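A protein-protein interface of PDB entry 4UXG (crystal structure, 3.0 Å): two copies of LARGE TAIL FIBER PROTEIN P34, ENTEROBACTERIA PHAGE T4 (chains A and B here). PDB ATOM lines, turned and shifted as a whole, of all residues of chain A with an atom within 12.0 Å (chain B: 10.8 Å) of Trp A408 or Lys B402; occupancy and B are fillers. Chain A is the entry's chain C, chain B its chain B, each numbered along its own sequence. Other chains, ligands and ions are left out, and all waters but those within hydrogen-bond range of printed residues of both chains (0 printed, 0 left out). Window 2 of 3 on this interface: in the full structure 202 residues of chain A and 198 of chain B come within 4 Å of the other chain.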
ATOM      1  N   PHE A 387       1.671  -2.691 -17.633  1.00  0.00           N
ATOM      2  CA  PHE A 387       0.556  -2.764 -16.690  1.00  0.00           C
ATOM      3  C   PHE A 387       0.621  -1.801 -15.512  1.00  0.00           C
ATOM      4  O   PHE A 387       1.690  -1.383 -15.090  1.00  0.00           O
ATOM      5  CB  PHE A 387       0.411  -4.196 -16.174  1.00  0.00           C
ATOM      6  CG  PHE A 387       1.559  -4.668 -15.338  1.00  0.00           C
ATOM      7  CD1 PHE A 387       1.619  -4.399 -13.978  1.00  0.00           C
ATOM      8  CD2 PHE A 387       2.566  -5.421 -15.915  1.00  0.00           C
ATOM      9  CE1 PHE A 387       2.678  -4.855 -13.218  1.00  0.00           C
ATOM     10  CE2 PHE A 387       3.623  -5.883 -15.165  1.00  0.00           C
ATOM     11  CZ  PHE A 387       3.682  -5.600 -13.814  1.00  0.00           C
ATOM     12  N   LEU A 388      -0.552  -1.478 -14.974  1.00  0.00           N
ATOM     13  CA  LEU A 388      -0.660  -0.632 -13.790  1.00  0.00           C
ATOM     14  C   LEU A 388      -1.429  -1.334 -12.691  1.00  0.00           C
ATOM     15  O   LEU A 388      -2.609  -1.622 -12.842  1.00  0.00           O
ATOM     16  CB  LEU A 388      -1.353   0.689 -14.128  1.00  0.00           C
ATOM     17  CG  LEU A 388      -1.832   1.524 -12.937  1.00  0.00           C
ATOM     18  CD1 LEU A 388      -0.662   1.951 -12.068  1.00  0.00           C
ATOM     19  CD2 LEU A 388      -2.627   2.741 -13.395  1.00  0.00           C
ATOM     20  N   ARG A 389      -0.771  -1.573 -11.569  1.00  0.00           N
ATOM     21  CA  ARG A 389      -1.415  -2.243 -10.455  1.00  0.00           C
ATOM     22  C   ARG A 389      -1.817  -1.266  -9.360  1.00  0.00           C
ATOM     23  O   ARG A 389      -1.027  -0.415  -8.956  1.00  0.00           O
ATOM     24  CB  ARG A 389      -0.483  -3.317  -9.898  1.00  0.00           C
ATOM     25  CG  ARG A 389      -1.018  -4.057  -8.693  1.00  0.00           C
ATOM     26  CD  ARG A 389      -0.165  -5.277  -8.394  1.00  0.00           C
ATOM     27  NE  ARG A 389      -0.473  -5.854  -7.090  1.00  0.00           N
ATOM     28  CZ  ARG A 389       0.068  -6.975  -6.626  1.00  0.00           C
ATOM     29  NH1 ARG A 389       0.937  -7.649  -7.367  1.00  0.00           N
ATOM     30  NH2 ARG A 389      -0.267  -7.427  -5.426  1.00  0.00           N
ATOM     31  N   ILE A 390      -3.047  -1.394  -8.874  1.00  0.00           N
ATOM     32  CA  ILE A 390      -3.502  -0.583  -7.752  1.00  0.00           C
ATOM     33  C   ILE A 390      -3.998  -1.523  -6.662  1.00  0.00           C
ATOM     34  O   ILE A 390      -5.063  -2.127  -6.776  1.00  0.00           O
ATOM     35  CB  ILE A 390      -4.615   0.410  -8.142  1.00  0.00           C
ATOM     36  CG1 ILE A 390      -4.150   1.332  -9.268  1.00  0.00           C
ATOM     37  CG2 ILE A 390      -5.012   1.255  -6.949  1.00  0.00           C
ATOM     38  CD1 ILE A 390      -4.571   0.883 -10.634  1.00  0.00           C
ATOM     39  N   GLY A 391      -3.208  -1.628  -5.600  1.00  0.00           N
ATOM     40  CA  GLY A 391      -3.439  -2.603  -4.554  1.00  0.00           C
ATOM     41  C   GLY A 391      -3.284  -4.017  -5.074  1.00  0.00           C
ATOM     42  O   GLY A 391      -2.175  -4.463  -5.368  1.00  0.00           O
ATOM     43  N   ASN A 392      -4.401  -4.721  -5.206  1.00  0.00           N
ATOM     44  CA  ASN A 392      -4.387  -6.100  -5.680  1.00  0.00           C
ATOM     45  C   ASN A 392      -4.995  -6.248  -7.075  1.00  0.00           C
ATOM     46  O   ASN A 392      -5.151  -7.362  -7.582  1.00  0.00           O
ATOM     47  CB  ASN A 392      -5.101  -7.001  -4.672  1.00  0.00           C
ATOM     48  CG  ASN A 392      -6.410  -6.413  -4.186  1.00  0.00           C
ATOM     49  OD1 ASN A 392      -6.634  -5.206  -4.281  1.00  0.00           O
ATOM     50  ND2 ASN A 392      -7.272  -7.262  -3.635  1.00  0.00           N
ATOM     51  N   VAL A 393      -5.341  -5.116  -7.683  1.00  0.00           N
ATOM     52  CA  VAL A 393      -5.968  -5.100  -9.001  1.00  0.00           C
ATOM     53  C   VAL A 393      -4.995  -4.684 -10.099  1.00  0.00           C
ATOM     54  O   VAL A 393      -4.558  -3.536 -10.143  1.00  0.00           O
ATOM     55  CB  VAL A 393      -7.161  -4.135  -9.033  1.00  0.00           C
ATOM     56  CG1 VAL A 393      -7.869  -4.206 -10.380  1.00  0.00           C
ATOM     57  CG2 VAL A 393      -8.112  -4.447  -7.905  1.00  0.00           C
ATOM     58  N   ARG A 394      -4.667  -5.610 -10.993  1.00  0.00           N
ATOM     59  CA  ARG A 394      -3.829  -5.276 -12.141  1.00  0.00           C
ATOM     60  C   ARG A 394      -4.664  -4.759 -13.305  1.00  0.00           C
ATOM     61  O   ARG A 394      -5.768  -5.236 -13.549  1.00  0.00           O
ATOM     62  CB  ARG A 394      -3.001  -6.480 -12.591  1.00  0.00           C
ATOM     63  CG  ARG A 394      -1.829  -6.774 -11.692  1.00  0.00           C
ATOM     64  CD  ARG A 394      -1.120  -8.063 -12.059  1.00  0.00           C
ATOM     65  NE  ARG A 394       0.069  -8.237 -11.227  1.00  0.00           N
ATOM     66  CZ  ARG A 394       0.869  -9.297 -11.263  1.00  0.00           C
ATOM     67  NH1 ARG A 394       0.614 -10.297 -12.096  1.00  0.00           N
ATOM     68  NH2 ARG A 394       1.925  -9.356 -10.460  1.00  0.00           N
ATOM     69  N   ILE A 395      -4.125  -3.773 -14.009  1.00  0.00           N
ATOM     70  CA  ILE A 395      -4.753  -3.213 -15.196  1.00  0.00           C
ATOM     71  C   ILE A 395      -3.814  -3.383 -16.380  1.00  0.00           C
ATOM     72  O   ILE A 395      -2.773  -2.726 -16.456  1.00  0.00           O
ATOM     73  CB  ILE A 395      -5.088  -1.723 -15.029  1.00  0.00           C
ATOM     74  CG1 ILE A 395      -6.101  -1.514 -13.907  1.00  0.00           C
ATOM     75  CG2 ILE A 395      -5.622  -1.153 -16.323  1.00  0.00           C
ATOM     76  CD1 ILE A 395      -6.363  -0.053 -13.609  1.00  0.00           C
ATOM     77  N   VAL A 396      -4.187  -4.257 -17.305  1.00  0.00           N
ATOM     78  CA  VAL A 396      -3.293  -4.625 -18.396  1.00  0.00           C
ATOM     79  C   VAL A 396      -3.880  -4.306 -19.763  1.00  0.00           C
ATOM     80  O   VAL A 396      -4.925  -4.833 -20.135  1.00  0.00           O
ATOM     81  CB  VAL A 396      -2.950  -6.122 -18.352  1.00  0.00           C
ATOM     82  CG1 VAL A 396      -2.024  -6.484 -19.506  1.00  0.00           C
ATOM     83  CG2 VAL A 396      -2.320  -6.479 -17.017  1.00  0.00           C
ATOM     84  N   VAL A 404      -8.610  -3.039 -22.204  1.00  0.00           N
ATOM     85  CA  VAL A 404      -7.807  -3.199 -21.006  1.00  0.00           C
ATOM     86  C   VAL A 404      -8.501  -4.255 -20.149  1.00  0.00           C
ATOM     87  O   VAL A 404      -9.724  -4.375 -20.181  1.00  0.00           O
ATOM     88  CB  VAL A 404      -7.644  -1.858 -20.255  1.00  0.00           C
ATOM     89  CG1 VAL A 404      -8.327  -0.740 -21.020  1.00  0.00           C
ATOM     90  CG2 VAL A 404      -8.199  -1.940 -18.846  1.00  0.00           C
ATOM     91  N   LYS A 405      -7.728  -5.022 -19.389  1.00  0.00           N
ATOM     92  CA  LYS A 405      -8.285  -6.097 -18.573  1.00  0.00           C
ATOM     93  C   LYS A 405      -7.901  -5.939 -17.102  1.00  0.00           C
ATOM     94  O   LYS A 405      -6.821  -5.441 -16.778  1.00  0.00           O
ATOM     95  CB  LYS A 405      -7.868  -7.460 -19.132  1.00  0.00           C
ATOM     96  CG  LYS A 405      -6.386  -7.650 -19.347  1.00  0.00           C
ATOM     97  CD  LYS A 405      -6.111  -9.033 -19.909  1.00  0.00           C
ATOM     98  CE  LYS A 405      -6.704  -9.170 -21.303  1.00  0.00           C
ATOM     99  NZ  LYS A 405      -6.358 -10.466 -21.952  1.00  0.00           N
ATOM    100  N   PHE A 406      -8.815  -6.347 -16.225  1.00  0.00           N
ATOM    101  CA  PHE A 406      -8.667  -6.204 -14.777  1.00  0.00           C
ATOM    102  C   PHE A 406      -8.457  -7.523 -14.025  1.00  0.00           C
ATOM    103  O   PHE A 406      -9.392  -8.303 -13.865  1.00  0.00           O
ATOM    104  CB  PHE A 406      -9.911  -5.518 -14.198  1.00  0.00           C
ATOM    105  CG  PHE A 406     -10.057  -4.069 -14.582  1.00  0.00           C
ATOM    106  CD1 PHE A 406     -10.199  -3.694 -15.908  1.00  0.00           C
ATOM    107  CD2 PHE A 406     -10.083  -3.084 -13.610  1.00  0.00           C
ATOM    108  CE1 PHE A 406     -10.345  -2.367 -16.255  1.00  0.00           C
ATOM    109  CE2 PHE A 406     -10.227  -1.752 -13.953  1.00  0.00           C
ATOM    110  CZ  PHE A 406     -10.358  -1.394 -15.278  1.00  0.00           C
ATOM    111  N   GLU A 407      -7.240  -7.754 -13.538  1.00  0.00           N
ATOM    112  CA  GLU A 407      -6.881  -9.023 -12.898  1.00  0.00           C
ATOM    113  C   GLU A 407      -6.735  -8.863 -11.390  1.00  0.00           C
ATOM    114  O   GLU A 407      -6.683  -7.743 -10.874  1.00  0.00           O
ATOM    115  CB  GLU A 407      -5.581  -9.597 -13.470  1.00  0.00           C
ATOM    116  CG  GLU A 407      -5.688 -10.191 -14.860  1.00  0.00           C
ATOM    117  CD  GLU A 407      -5.482  -9.170 -15.955  1.00  0.00           C
ATOM    118  OE1 GLU A 407      -5.830  -7.991 -15.746  1.00  0.00           O
ATOM    119  OE2 GLU A 407      -4.961  -9.548 -17.024  1.00  0.00           O
ATOM    120  N   TRP A 408      -6.656  -9.993 -10.694  1.00  0.00           N
ATOM    121  CA  TRP A 408      -6.465 -10.002  -9.247  1.00  0.00           C
ATOM    122  C   TRP A 408      -5.329 -10.932  -8.830  1.00  0.00           C
ATOM    123  O   TRP A 408      -4.499 -10.577  -7.993  1.00  0.00           O
ATOM    124  CB  TRP A 408      -7.760 -10.437  -8.567  1.00  0.00           C
ATOM    125  CG  TRP A 408      -8.871  -9.448  -8.705  1.00  0.00           C
ATOM    126  CD1 TRP A 408      -9.734  -9.338  -9.756  1.00  0.00           C
ATOM    127  CD2 TRP A 408      -9.286  -8.475  -7.742  1.00  0.00           C
ATOM    128  NE1 TRP A 408     -10.637  -8.332  -9.525  1.00  0.00           N
ATOM    129  CE2 TRP A 408     -10.390  -7.788  -8.292  1.00  0.00           C
ATOM    130  CE3 TRP A 408      -8.827  -8.104  -6.474  1.00  0.00           C
ATOM    131  CZ2 TRP A 408     -11.039  -6.756  -7.620  1.00  0.00           C
ATOM    132  CZ3 TRP A 408      -9.474  -7.076  -5.808  1.00  0.00           C
ATOM    133  CH2 TRP A 408     -10.568  -6.416  -6.383  1.00  0.00           C
ATOM    134  N   THR B 383       3.328   0.116  -9.627  1.00  0.00           N
ATOM    135  CA  THR B 383       2.457  -0.499  -8.632  1.00  0.00           C
ATOM    136  C   THR B 383       2.114   0.507  -7.537  1.00  0.00           C
ATOM    137  O   THR B 383       2.999   1.150  -6.981  1.00  0.00           O
ATOM    138  CB  THR B 383       3.114  -1.740  -7.991  1.00  0.00           C
ATOM    139  OG1 THR B 383       3.399  -2.717  -8.999  1.00  0.00           O
ATOM    140  CG2 THR B 383       2.205  -2.348  -6.933  1.00  0.00           C
ATOM    141  N   ILE B 395      -8.680   6.562  -6.178  1.00  0.00           N
ATOM    142  CA  ILE B 395      -8.888   5.130  -6.332  1.00  0.00           C
ATOM    143  C   ILE B 395      -8.224   4.382  -5.179  1.00  0.00           C
ATOM    144  O   ILE B 395      -6.994   4.346  -5.082  1.00  0.00           O
ATOM    145  CB  ILE B 395      -8.311   4.628  -7.663  1.00  0.00           C
ATOM    146  CG1 ILE B 395      -8.962   5.358  -8.838  1.00  0.00           C
ATOM    147  CG2 ILE B 395      -8.447   3.117  -7.774  1.00  0.00           C
ATOM    148  CD1 ILE B 395      -8.336   5.029 -10.173  1.00  0.00           C
ATOM    149  N   VAL B 396      -9.034   3.783  -4.313  1.00  0.00           N
ATOM    150  CA  VAL B 396      -8.525   3.179  -3.087  1.00  0.00           C
ATOM    151  C   VAL B 396      -8.821   1.686  -3.009  1.00  0.00           C
ATOM    152  O   VAL B 396      -9.975   1.284  -2.945  1.00  0.00           O
ATOM    153  CB  VAL B 396      -9.135   3.856  -1.848  1.00  0.00           C
ATOM    154  CG1 VAL B 396      -8.598   3.216  -0.577  1.00  0.00           C
ATOM    155  CG2 VAL B 396      -8.855   5.350  -1.866  1.00  0.00           C
ATOM    156  N   PRO B 397      -7.773   0.855  -2.978  1.00  0.00           N
ATOM    157  CA  PRO B 397      -7.944  -0.589  -2.779  1.00  0.00           C
ATOM    158  C   PRO B 397      -8.401  -0.934  -1.364  1.00  0.00           C
ATOM    159  O   PRO B 397      -8.028  -0.252  -0.412  1.00  0.00           O
ATOM    160  CB  PRO B 397      -6.545  -1.154  -3.047  1.00  0.00           C
ATOM    161  CG  PRO B 397      -5.842  -0.101  -3.821  1.00  0.00           C
ATOM    162  CD  PRO B 397      -6.391   1.201  -3.341  1.00  0.00           C
ATOM    163  N   ASP B 398      -9.215  -1.978  -1.240  1.00  0.00           N
ATOM    164  CA  ASP B 398      -9.609  -2.494   0.068  1.00  0.00           C
ATOM    165  C   ASP B 398      -9.129  -3.931   0.270  1.00  0.00           C
ATOM    166  O   ASP B 398      -9.774  -4.874  -0.187  1.00  0.00           O
ATOM    167  CB  ASP B 398     -11.129  -2.422   0.229  1.00  0.00           C
ATOM    168  CG  ASP B 398     -11.582  -2.737   1.641  1.00  0.00           C
ATOM    169  OD1 ASP B 398     -10.816  -2.465   2.588  1.00  0.00           O
ATOM    170  OD2 ASP B 398     -12.703  -3.265   1.803  1.00  0.00           O
ATOM    171  N   PRO B 399      -7.984  -4.093   0.955  1.00  0.00           N
ATOM    172  CA  PRO B 399      -7.251  -5.359   1.102  1.00  0.00           C
ATOM    173  C   PRO B 399      -8.006  -6.456   1.857  1.00  0.00           C
ATOM    174  O   PRO B 399      -7.779  -7.636   1.581  1.00  0.00           O
ATOM    175  CB  PRO B 399      -5.999  -4.943   1.880  1.00  0.00           C
ATOM    176  CG  PRO B 399      -6.412  -3.732   2.633  1.00  0.00           C
ATOM    177  CD  PRO B 399      -7.349  -3.005   1.719  1.00  0.00           C
ATOM    178  N   VAL B 400      -8.882  -6.082   2.789  1.00  0.00           N
ATOM    179  CA  VAL B 400      -9.607  -7.069   3.587  1.00  0.00           C
ATOM    180  C   VAL B 400     -10.485  -7.923   2.675  1.00  0.00           C
ATOM    181  O   VAL B 400     -10.469  -9.152   2.758  1.00  0.00           O
ATOM    182  CB  VAL B 400     -10.456  -6.400   4.701  1.00  0.00           C
ATOM    183  CG1 VAL B 400     -11.237  -5.203   4.165  1.00  0.00           C
ATOM    184  CG2 VAL B 400     -11.379  -7.416   5.363  1.00  0.00           C
ATOM    185  N   ASN B 401     -11.248  -7.269   1.807  1.00  0.00           N
ATOM    186  CA  ASN B 401     -12.040  -7.964   0.807  1.00  0.00           C
ATOM    187  C   ASN B 401     -11.312  -7.868  -0.525  1.00  0.00           C
ATOM    188  O   ASN B 401     -10.111  -7.609  -0.566  1.00  0.00           O
ATOM    189  CB  ASN B 401     -13.441  -7.361   0.693  1.00  0.00           C
ATOM    190  CG  ASN B 401     -14.198  -7.391   2.003  1.00  0.00           C
ATOM    191  OD1 ASN B 401     -13.665  -7.804   3.032  1.00  0.00           O
ATOM    192  ND2 ASN B 401     -15.453  -6.955   1.971  1.00  0.00           N
ATOM    193  N   LYS B 402     -12.037  -8.093  -1.611  1.00  0.00           N
ATOM    194  CA  LYS B 402     -11.492  -7.883  -2.945  1.00  0.00           C
ATOM    195  C   LYS B 402     -12.324  -6.767  -3.556  1.00  0.00           C
ATOM    196  O   LYS B 402     -13.313  -7.018  -4.242  1.00  0.00           O
ATOM    197  CB  LYS B 402     -11.521  -9.159  -3.791  1.00  0.00           C
ATOM    198  CG  LYS B 402     -10.745 -10.318  -3.180  1.00  0.00           C
ATOM    199  CD  LYS B 402     -10.777 -11.551  -4.068  1.00  0.00           C
ATOM    200  CE  LYS B 402      -9.958 -12.680  -3.463  1.00  0.00           C
ATOM    201  NZ  LYS B 402      -9.920 -13.888  -4.332  1.00  0.00           N
ATOM    202  N   THR B 403     -11.906  -5.530  -3.305  1.00  0.00           N
ATOM    203  CA  THR B 403     -12.737  -4.372  -3.603  1.00  0.00           C
ATOM    204  C   THR B 403     -11.892  -3.136  -3.911  1.00  0.00           C
ATOM    205  O   THR B 403     -10.759  -3.007  -3.446  1.00  0.00           O
ATOM    206  CB  THR B 403     -13.680  -4.067  -2.404  1.00  0.00           C
ATOM    207  OG1 THR B 403     -14.426  -5.242  -2.066  1.00  0.00           O
ATOM    208  CG2 THR B 403     -14.641  -2.919  -2.699  1.00  0.00           C
ATOM    209  N   VAL B 404     -12.458  -2.243  -4.719  1.00  0.00           N
ATOM    210  CA  VAL B 404     -11.871  -0.946  -5.014  1.00  0.00           C
ATOM    211  C   VAL B 404     -12.923   0.128  -4.746  1.00  0.00           C
ATOM    212  O   VAL B 404     -14.115  -0.124  -4.892  1.00  0.00           O
ATOM    213  CB  VAL B 404     -11.395  -0.868  -6.482  1.00  0.00           C
ATOM    214  CG1 VAL B 404     -10.777   0.487  -6.795  1.00  0.00           C
ATOM    215  CG2 VAL B 404     -10.403  -1.974  -6.770  1.00  0.00           C
ATOM    216  N   LYS B 405     -12.485   1.317  -4.354  1.00  0.00           N
ATOM    217  CA  LYS B 405     -13.390   2.415  -4.061  1.00  0.00           C
ATOM    218  C   LYS B 405     -13.023   3.588  -4.944  1.00  0.00           C
ATOM    219  O   LYS B 405     -11.842   3.856  -5.173  1.00  0.00           O
ATOM    220  CB  LYS B 405     -13.293   2.857  -2.598  1.00  0.00           C
ATOM    221  CG  LYS B 405     -13.844   1.913  -1.549  1.00  0.00           C
ATOM    222  CD  LYS B 405     -13.543   2.487  -0.165  1.00  0.00           C
ATOM    223  CE  LYS B 405     -13.995   1.577   0.962  1.00  0.00           C
ATOM    224  NZ  LYS B 405     -13.743   2.206   2.293  1.00  0.00           N
ATOM    225  N   PHE B 406     -14.033   4.283  -5.445  1.00  0.00           N
ATOM    226  CA  PHE B 406     -13.801   5.483  -6.229  1.00  0.00           C
ATOM    227  C   PHE B 406     -14.358   6.679  -5.487  1.00  0.00           C
ATOM    228  O   PHE B 406     -15.562   6.913  -5.480  1.00  0.00           O
ATOM    229  CB  PHE B 406     -14.424   5.369  -7.618  1.00  0.00           C
ATOM    230  CG  PHE B 406     -13.697   4.429  -8.534  1.00  0.00           C
ATOM    231  CD1 PHE B 406     -13.562   3.086  -8.219  1.00  0.00           C
ATOM    232  CD2 PHE B 406     -13.143   4.892  -9.714  1.00  0.00           C
ATOM    233  CE1 PHE B 406     -12.890   2.224  -9.064  1.00  0.00           C
ATOM    234  CE2 PHE B 406     -12.474   4.034 -10.565  1.00  0.00           C
ATOM    235  CZ  PHE B 406     -12.345   2.698 -10.239  1.00  0.00           C
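Positions printed for both chains: 395, 396, 404, 405 and 406.
Of the 7 pairs that touch across the chains among the printed residues, none has its exchanged pair printed and touching as well.
Among the printed residues, pairs that only touch across the chains: Trp A408 with Lys B402, Trp A408 with Thr B403, Arg A389 with Thr B383, Ile A390 with Pro B397, Gly A391 with Pro B397, Val A393 with Val B404 and Ile A390 with Ile B395.
N of Asp B398 lies within hydrogen-bond range of O of Thr B403 (2.9 Å).
The guanidinium group (NE) of Arg A389 lies within hydrogen-bond range of the backbone carbonyl oxygen (O) of Gly A391, 2.8 Å away.
Of the printed residues of chain B, Arg A389 touches Thr B383 (3.5 Å).
Printed residues of chain B within 4 Å of Gly A391: Pro B397.
Printed residues of chain B within 4 Å of Val A393: Val B404.
Glu A407 touches none of the printed residues of chain B.
Trp A408 touches just these residues of chain B: Lys B402 (3.3 Å) and Thr B403 (3.5 Å).
Of the printed residues of chain A, Thr B383 touches Arg A389 (3.5 Å).
Asp B398 touches none of the printed residues of chain A.
Of the 13 printed residues of chain B, 6 touch a printed residue of chain A.
Printed residues of chain B that touch a printed residue of chain A: Thr B383, Ile B395, Pro B397, Lys B402, Thr B403 and Val B404.
Along chain A the printed residues that touch a printed residue of chain B span positions 389 to 408.
Among the printed residues, no Asp or Glu carboxylate lies within 4 Å of a Lys or Arg side-chain nitrogen of the other chain.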
